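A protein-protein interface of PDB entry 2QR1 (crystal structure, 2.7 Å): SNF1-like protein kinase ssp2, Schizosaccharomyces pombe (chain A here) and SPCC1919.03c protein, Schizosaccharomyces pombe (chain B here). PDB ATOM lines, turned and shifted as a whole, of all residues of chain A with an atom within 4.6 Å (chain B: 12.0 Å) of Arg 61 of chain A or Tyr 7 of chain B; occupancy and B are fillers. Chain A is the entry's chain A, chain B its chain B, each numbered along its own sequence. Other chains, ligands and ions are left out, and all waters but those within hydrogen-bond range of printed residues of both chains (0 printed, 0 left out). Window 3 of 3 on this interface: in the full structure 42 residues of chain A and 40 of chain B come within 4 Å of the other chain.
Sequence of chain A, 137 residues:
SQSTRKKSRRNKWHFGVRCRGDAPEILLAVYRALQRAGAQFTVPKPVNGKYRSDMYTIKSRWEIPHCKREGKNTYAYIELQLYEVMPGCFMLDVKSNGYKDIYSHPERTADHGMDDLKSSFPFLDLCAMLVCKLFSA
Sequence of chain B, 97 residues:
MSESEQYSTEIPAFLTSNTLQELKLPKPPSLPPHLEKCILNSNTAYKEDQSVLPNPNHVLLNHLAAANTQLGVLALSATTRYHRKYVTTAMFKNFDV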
ATOM      1  N   ALA A  39     -29.879  -1.910  13.883  1.00  0.00           N
ATOM      2  CA  ALA A  39     -28.809  -1.396  13.069  1.00  0.00           C
ATOM      3  C   ALA A  39     -28.464  -0.013  13.620  1.00  0.00           C
ATOM      4  O   ALA A  39     -29.235   0.576  14.400  1.00  0.00           O
ATOM      5  CB  ALA A  39     -29.246  -1.327  11.619  1.00  0.00           C
ATOM      6  N   GLN A  40     -27.289   0.488  13.251  1.00  0.00           N
ATOM      7  CA  GLN A  40     -26.898   1.829  13.635  1.00  0.00           C
ATOM      8  C   GLN A  40     -26.657   2.559  12.354  1.00  0.00           C
ATOM      9  O   GLN A  40     -26.478   1.924  11.342  1.00  0.00           O
ATOM     10  CB  GLN A  40     -25.683   1.799  14.537  1.00  0.00           C
ATOM     11  CG  GLN A  40     -25.964   1.028  15.830  1.00  0.00           C
ATOM     12  CD  GLN A  40     -24.932   1.289  16.884  1.00  0.00           C
ATOM     13  OE1 GLN A  40     -24.028   2.092  16.677  1.00  0.00           O
ATOM     14  NE2 GLN A  40     -25.052   0.614  18.031  1.00  0.00           N
ATOM     15  N   PHE A  41     -26.689   3.884  12.384  1.00  0.00           N
ATOM     16  CA  PHE A  41     -26.849   4.664  11.167  1.00  0.00           C
ATOM     17  C   PHE A  41     -26.282   6.071  11.266  1.00  0.00           C
ATOM     18  O   PHE A  41     -26.245   6.665  12.349  1.00  0.00           O
ATOM     19  CB  PHE A  41     -28.330   4.748  10.791  1.00  0.00           C
ATOM     20  CG  PHE A  41     -29.263   4.870  11.978  1.00  0.00           C
ATOM     21  CD1 PHE A  41     -29.519   6.098  12.564  1.00  0.00           C
ATOM     22  CD2 PHE A  41     -29.895   3.750  12.500  1.00  0.00           C
ATOM     23  CE1 PHE A  41     -30.378   6.212  13.653  1.00  0.00           C
ATOM     24  CE2 PHE A  41     -30.756   3.870  13.593  1.00  0.00           C
ATOM     25  CZ  PHE A  41     -30.990   5.107  14.168  1.00  0.00           C
ATOM     26  N   THR A  42     -25.857   6.601  10.118  1.00  0.00           N
ATOM     27  CA  THR A  42     -25.553   8.012  10.017  1.00  0.00           C
ATOM     28  C   THR A  42     -26.850   8.794   9.961  1.00  0.00           C
ATOM     29  O   THR A  42     -27.936   8.251   9.752  1.00  0.00           O
ATOM     30  CB  THR A  42     -24.766   8.372   8.763  1.00  0.00           C
ATOM     31  OG1 THR A  42     -25.597   8.153   7.633  1.00  0.00           O
ATOM     32  CG2 THR A  42     -23.509   7.550   8.638  1.00  0.00           C
ATOM     33  N   LYS A  59     -25.852   5.455   5.590  1.00  0.00           N
ATOM     34  CA  LYS A  59     -24.921   4.362   5.826  1.00  0.00           C
ATOM     35  C   LYS A  59     -25.297   3.676   7.130  1.00  0.00           C
ATOM     36  O   LYS A  59     -25.369   4.319   8.164  1.00  0.00           O
ATOM     37  CB  LYS A  59     -23.494   4.896   5.903  1.00  0.00           C
ATOM     38  CG  LYS A  59     -22.998   5.514   4.611  1.00  0.00           C
ATOM     39  CD  LYS A  59     -21.530   5.221   4.459  1.00  0.00           C
ATOM     40  CE  LYS A  59     -20.935   5.907   3.264  1.00  0.00           C
ATOM     41  NZ  LYS A  59     -19.475   5.702   3.365  1.00  0.00           N
ATOM     42  N   SER A  60     -25.556   2.389   7.104  1.00  0.00           N
ATOM     43  CA  SER A  60     -25.891   1.716   8.348  1.00  0.00           C
ATOM     44  C   SER A  60     -24.834   0.668   8.683  1.00  0.00           C
ATOM     45  O   SER A  60     -24.039   0.284   7.830  1.00  0.00           O
ATOM     46  CB  SER A  60     -27.302   1.088   8.302  1.00  0.00           C
ATOM     47  OG  SER A  60     -27.388   0.014   7.366  1.00  0.00           O
ATOM     48  N   ARG A  61     -24.827   0.213   9.924  1.00  0.00           N
ATOM     49  CA  ARG A  61     -23.960  -0.859  10.354  1.00  0.00           C
ATOM     50  C   ARG A  61     -24.752  -1.848  11.194  1.00  0.00           C
ATOM     51  O   ARG A  61     -25.466  -1.473  12.147  1.00  0.00           O
ATOM     52  CB  ARG A  61     -22.822  -0.292  11.168  1.00  0.00           C
ATOM     53  CG  ARG A  61     -21.704  -1.259  11.436  1.00  0.00           C
ATOM     54  CD  ARG A  61     -20.648  -0.603  12.250  1.00  0.00           C
ATOM     55  NE  ARG A  61     -21.041  -0.448  13.641  1.00  0.00           N
ATOM     56  CZ  ARG A  61     -20.439   0.390  14.480  1.00  0.00           C
ATOM     57  NH1 ARG A  61     -19.424   1.142  14.054  1.00  0.00           N
ATOM     58  NH2 ARG A  61     -20.841   0.480  15.742  1.00  0.00           N
ATOM     59  N   TRP A  62     -24.609  -3.114  10.841  1.00  0.00           N
ATOM     60  CA  TRP A  62     -25.409  -4.171  11.409  1.00  0.00           C
ATOM     61  C   TRP A  62     -24.498  -5.205  12.061  1.00  0.00           C
ATOM     62  O   TRP A  62     -23.521  -5.661  11.451  1.00  0.00           O
ATOM     63  CB  TRP A  62     -26.189  -4.834  10.300  1.00  0.00           C
ATOM     64  CG  TRP A  62     -27.203  -3.951   9.557  1.00  0.00           C
ATOM     65  CD1 TRP A  62     -26.947  -2.882   8.716  1.00  0.00           C
ATOM     66  CD2 TRP A  62     -28.616  -4.130   9.545  1.00  0.00           C
ATOM     67  NE1 TRP A  62     -28.125  -2.382   8.208  1.00  0.00           N
ATOM     68  CE2 TRP A  62     -29.163  -3.121   8.706  1.00  0.00           C
ATOM     69  CE3 TRP A  62     -29.478  -5.037  10.175  1.00  0.00           C
ATOM     70  CZ2 TRP A  62     -30.541  -2.998   8.481  1.00  0.00           C
ATOM     71  CZ3 TRP A  62     -30.842  -4.924   9.950  1.00  0.00           C
ATOM     72  CH2 TRP A  62     -31.366  -3.905   9.106  1.00  0.00           C
ATOM     73  N   GLU A  63     -24.793  -5.542  13.311  1.00  0.00           N
ATOM     74  CA  GLU A  63     -24.052  -6.570  14.015  1.00  0.00           C
ATOM     75  C   GLU A  63     -24.556  -7.880  13.438  1.00  0.00           C
ATOM     76  O   GLU A  63     -25.753  -8.073  13.336  1.00  0.00           O
ATOM     77  CB  GLU A  63     -24.316  -6.471  15.522  1.00  0.00           C
ATOM     78  CG  GLU A  63     -23.218  -7.110  16.383  1.00  0.00           C
ATOM     79  CD  GLU A  63     -22.920  -6.359  17.705  1.00  0.00           C
ATOM     80  OE1 GLU A  63     -23.878  -5.862  18.354  1.00  0.00           O
ATOM     81  OE2 GLU A  63     -21.722  -6.289  18.101  1.00  0.00           O
ATOM     82  N   TYR A  75     -19.226  -7.034  11.589  1.00  0.00           N
ATOM     83  CA  TYR A  75     -20.253  -6.054  11.263  1.00  0.00           C
ATOM     84  C   TYR A  75     -20.570  -6.157   9.794  1.00  0.00           C
ATOM     85  O   TYR A  75     -19.753  -6.661   9.030  1.00  0.00           O
ATOM     86  CB  TYR A  75     -19.768  -4.636  11.611  1.00  0.00           C
ATOM     87  CG  TYR A  75     -19.647  -4.392  13.106  1.00  0.00           C
ATOM     88  CD1 TYR A  75     -18.494  -4.738  13.798  1.00  0.00           C
ATOM     89  CD2 TYR A  75     -20.699  -3.826  13.827  1.00  0.00           C
ATOM     90  CE1 TYR A  75     -18.384  -4.522  15.155  1.00  0.00           C
ATOM     91  CE2 TYR A  75     -20.599  -3.607  15.188  1.00  0.00           C
ATOM     92  CZ  TYR A  75     -19.439  -3.958  15.844  1.00  0.00           C
ATOM     93  OH  TYR A  75     -19.329  -3.735  17.196  1.00  0.00           O
ATOM     94  N   ALA A  76     -21.757  -5.706   9.408  1.00  0.00           N
ATOM     95  CA  ALA A  76     -22.111  -5.618   8.004  1.00  0.00           C
ATOM     96  C   ALA A  76     -22.502  -4.175   7.648  1.00  0.00           C
ATOM     97  O   ALA A  76     -23.276  -3.527   8.348  1.00  0.00           O
ATOM     98  CB  ALA A  76     -23.213  -6.575   7.694  1.00  0.00           C
ATOM     99  N   TYR A  77     -21.946  -3.674   6.559  1.00  0.00           N
ATOM    100  CA  TYR A  77     -22.138  -2.305   6.154  1.00  0.00           C
ATOM    101  C   TYR A  77     -23.123  -2.212   4.988  1.00  0.00           C
ATOM    102  O   TYR A  77     -22.906  -2.763   3.900  1.00  0.00           O
ATOM    103  CB  TYR A  77     -20.775  -1.717   5.811  1.00  0.00           C
ATOM    104  CG  TYR A  77     -19.864  -1.688   7.029  1.00  0.00           C
ATOM    105  CD1 TYR A  77     -19.931  -0.638   7.933  1.00  0.00           C
ATOM    106  CD2 TYR A  77     -18.964  -2.729   7.298  1.00  0.00           C
ATOM    107  CE1 TYR A  77     -19.140  -0.618   9.049  1.00  0.00           C
ATOM    108  CE2 TYR A  77     -18.152  -2.701   8.426  1.00  0.00           C
ATOM    109  CZ  TYR A  77     -18.255  -1.645   9.287  1.00  0.00           C
ATOM    110  OH  TYR A  77     -17.490  -1.587  10.418  1.00  0.00           O
ATOM    111  N   GLN B   6     -19.374   8.354  11.019  1.00  0.00           N
ATOM    112  CA  GLN B   6     -19.857   8.546  12.381  1.00  0.00           C
ATOM    113  C   GLN B   6     -21.253   7.959  12.558  1.00  0.00           C
ATOM    114  O   GLN B   6     -22.244   8.552  12.131  1.00  0.00           O
ATOM    115  CB  GLN B   6     -19.859  10.032  12.745  1.00  0.00           C
ATOM    116  CG  GLN B   6     -18.523  10.726  12.535  1.00  0.00           C
ATOM    117  CD  GLN B   6     -17.700  10.801  13.806  1.00  0.00           C
ATOM    118  OE1 GLN B   6     -17.784   9.926  14.667  1.00  0.00           O
ATOM    119  NE2 GLN B   6     -16.898  11.853  13.930  1.00  0.00           N
ATOM    120  N   TYR B   7     -21.323   6.793  13.192  1.00  0.00           N
ATOM    121  CA  TYR B   7     -22.606   6.095  13.387  1.00  0.00           C
ATOM    122  C   TYR B   7     -23.456   6.632  14.551  1.00  0.00           C
ATOM    123  O   TYR B   7     -23.000   7.485  15.296  1.00  0.00           O
ATOM    124  CB  TYR B   7     -22.372   4.583  13.522  1.00  0.00           C
ATOM    125  CG  TYR B   7     -21.944   3.966  12.214  1.00  0.00           C
ATOM    126  CD1 TYR B   7     -20.638   3.540  12.012  1.00  0.00           C
ATOM    127  CD2 TYR B   7     -22.838   3.874  11.159  1.00  0.00           C
ATOM    128  CE1 TYR B   7     -20.241   3.022  10.811  1.00  0.00           C
ATOM    129  CE2 TYR B   7     -22.458   3.361   9.960  1.00  0.00           C
ATOM    130  CZ  TYR B   7     -21.160   2.932   9.789  1.00  0.00           C
ATOM    131  OH  TYR B   7     -20.817   2.397   8.570  1.00  0.00           O
ATOM    132  N   SER B   8     -24.697   6.148  14.679  1.00  0.00           N
ATOM    133  CA  SER B   8     -25.625   6.591  15.733  1.00  0.00           C
ATOM    134  C   SER B   8     -26.791   5.632  15.948  1.00  0.00           C
ATOM    135  O   SER B   8     -27.229   4.939  15.042  1.00  0.00           O
ATOM    136  CB  SER B   8     -26.173   7.995  15.438  1.00  0.00           C
ATOM    137  OG  SER B   8     -27.388   8.239  16.133  1.00  0.00           O
ATOM    138  N   THR B   9     -27.312   5.645  17.166  1.00  0.00           N
ATOM    139  CA  THR B   9     -28.379   4.741  17.575  1.00  0.00           C
ATOM    140  C   THR B   9     -29.774   5.391  17.624  1.00  0.00           C
ATOM    141  O   THR B   9     -30.782   4.677  17.647  1.00  0.00           O
ATOM    142  CB  THR B   9     -28.058   4.121  18.947  1.00  0.00           C
ATOM    143  OG1 THR B   9     -29.194   3.400  19.421  1.00  0.00           O
ATOM    144  CG2 THR B   9     -27.698   5.204  19.964  1.00  0.00           C
ATOM    145  N   GLU B  10     -29.835   6.727  17.632  1.00  0.00           N
ATOM    146  CA  GLU B  10     -31.111   7.428  17.830  1.00  0.00           C
ATOM    147  C   GLU B  10     -31.707   8.197  16.633  1.00  0.00           C
ATOM    148  O   GLU B  10     -30.983   8.834  15.865  1.00  0.00           O
ATOM    149  CB  GLU B  10     -31.038   8.323  19.067  1.00  0.00           C
ATOM    150  CG  GLU B  10     -31.026   7.551  20.411  1.00  0.00           C
ATOM    151  CD  GLU B  10     -32.248   6.637  20.634  1.00  0.00           C
ATOM    152  OE1 GLU B  10     -33.234   6.693  19.850  1.00  0.00           O
ATOM    153  OE2 GLU B  10     -32.215   5.862  21.616  1.00  0.00           O
ATOM    154  N   ILE B  11     -33.040   8.103  16.506  1.00  0.00           N
ATOM    155  CA  ILE B  11     -33.871   8.776  15.479  1.00  0.00           C
ATOM    156  C   ILE B  11     -33.688  10.298  15.425  1.00  0.00           C
ATOM    157  O   ILE B  11     -33.920  10.976  16.424  1.00  0.00           O
ATOM    158  CB  ILE B  11     -35.399   8.479  15.714  1.00  0.00           C
ATOM    159  CG1 ILE B  11     -35.726   8.307  17.218  1.00  0.00           C
ATOM    160  CG2 ILE B  11     -35.838   7.231  14.968  1.00  0.00           C
ATOM    161  CD1 ILE B  11     -36.063   9.605  18.009  1.00  0.00           C
ATOM    162  N   PRO B  12     -33.285  10.851  14.265  1.00  0.00           N
ATOM    163  CA  PRO B  12     -33.046  12.303  14.266  1.00  0.00           C
ATOM    164  C   PRO B  12     -34.295  13.035  14.722  1.00  0.00           C
ATOM    165  O   PRO B  12     -35.406  12.702  14.280  1.00  0.00           O
ATOM    166  CB  PRO B  12     -32.731  12.628  12.806  1.00  0.00           C
ATOM    167  CG  PRO B  12     -32.256  11.352  12.229  1.00  0.00           C
ATOM    168  CD  PRO B  12     -33.022  10.252  12.943  1.00  0.00           C
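N of Arg 61 of chain A lies within hydrogen-bond range of O of Gln 40 of chain A, 2.8 Å away.
The backbone NH (N) of Thr 42 of chain A sits at hydrogen-bond distance from the backbone carbonyl oxygen (O) of Lys 59 of chain A, 3.0 Å away.
NE1 of Trp 62 of chain A sits at hydrogen-bond distance from OG of Ser 60 of chain A.
N of Glu 10 of chain B lies within hydrogen-bond range of OG of Ser 8 of chain B, at 3.2 Å.
Of the printed residues of chain B, Arg 61 of chain A touches Tyr 7.
Of chain A, only Phe 41 (3.6 Å), Lys 59 (3.6 Å), Ser 60 (3.8 Å), Arg 61 (3.4 Å) and Tyr 77 (3.2 Å) come within 4 Å of Tyr 7 of chain B.
No residue of chain B comes within 4 Å of Ala 39 of chain A.
Gln 40 of chain A touches just one residue of chain B: Ser 8.
Phe 41 of chain A touches four residues of chain B.
Of chain B, only Gln 6 comes within 4 Å of Thr 42 of chain A.
Of the printed residues of chain B, Lys 59 of chain A touches Tyr 7 (3.6 Å).
Ala 76 of chain A touches none of the printed residues of chain B.
Tyr 77 of chain A touches just one residue of chain B: Tyr 7 (3.2 Å).
Of the printed residues of chain A, Glu 10 of chain B touches Phe 41 (3.5 Å).
Printed residues of chain A within 4 Å of Gln 6 of chain B: Thr 42.
Printed residues of chain A within 4 Å of Thr 9 of chain B: Phe 41.
Printed residues of chain A within 4 Å of Ser 8 of chain B: Gln 40 and Phe 41.
Pro 12 of chain B touches none of the printed residues of chain A.
The nearest residue of chain A that does not touch Tyr 7 of chain B is Gln 40 of chain A (4.1 Å).
The nearest printed residue of chain A that does not touch Thr 9 of chain B is Gln 40 of chain A (4.7 Å).
Printed residues of chain B that touch a printed residue of chain A: Gln 6, Tyr 7, Ser 8, Thr 9 and Glu 10.
Among the printed residues, 10 pairs touch across the chains.
Gln 40 of chain A touches Ser 8 of chain B (CA to O, 3.4 Å).
Tyr 7 of chain B touches Phe 41 of chain A (C to O, 3.6 Å).
CZ of Phe 41 of chain A touches O of Thr 9 of chain B, at 3.5 Å.
Phe 41 of chain A touches Glu 10 of chain B (CE1 to O, 3.5 Å).
O of Gln 6 of chain B touches CG2 of Thr 42 of chain A (3.8 Å).
Lys 59 of chain A touches Tyr 7 of chain B.
Tyr 7 of chain B touches Ser 60 of chain A.
Tyr 7 of chain B touches Arg 61 of chain A (CD1 to NH1, 3.4 Å).
Tyr 77 of chain A touches Tyr 7 of chain B (CD1 to OH, 3.2 Å).
The backbone carbonyl oxygen (O) of Phe 41 of chain A sits at hydrogen-bond distance from the backbone NH (N) of Ser 8 of chain B, at 2.8 Å.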
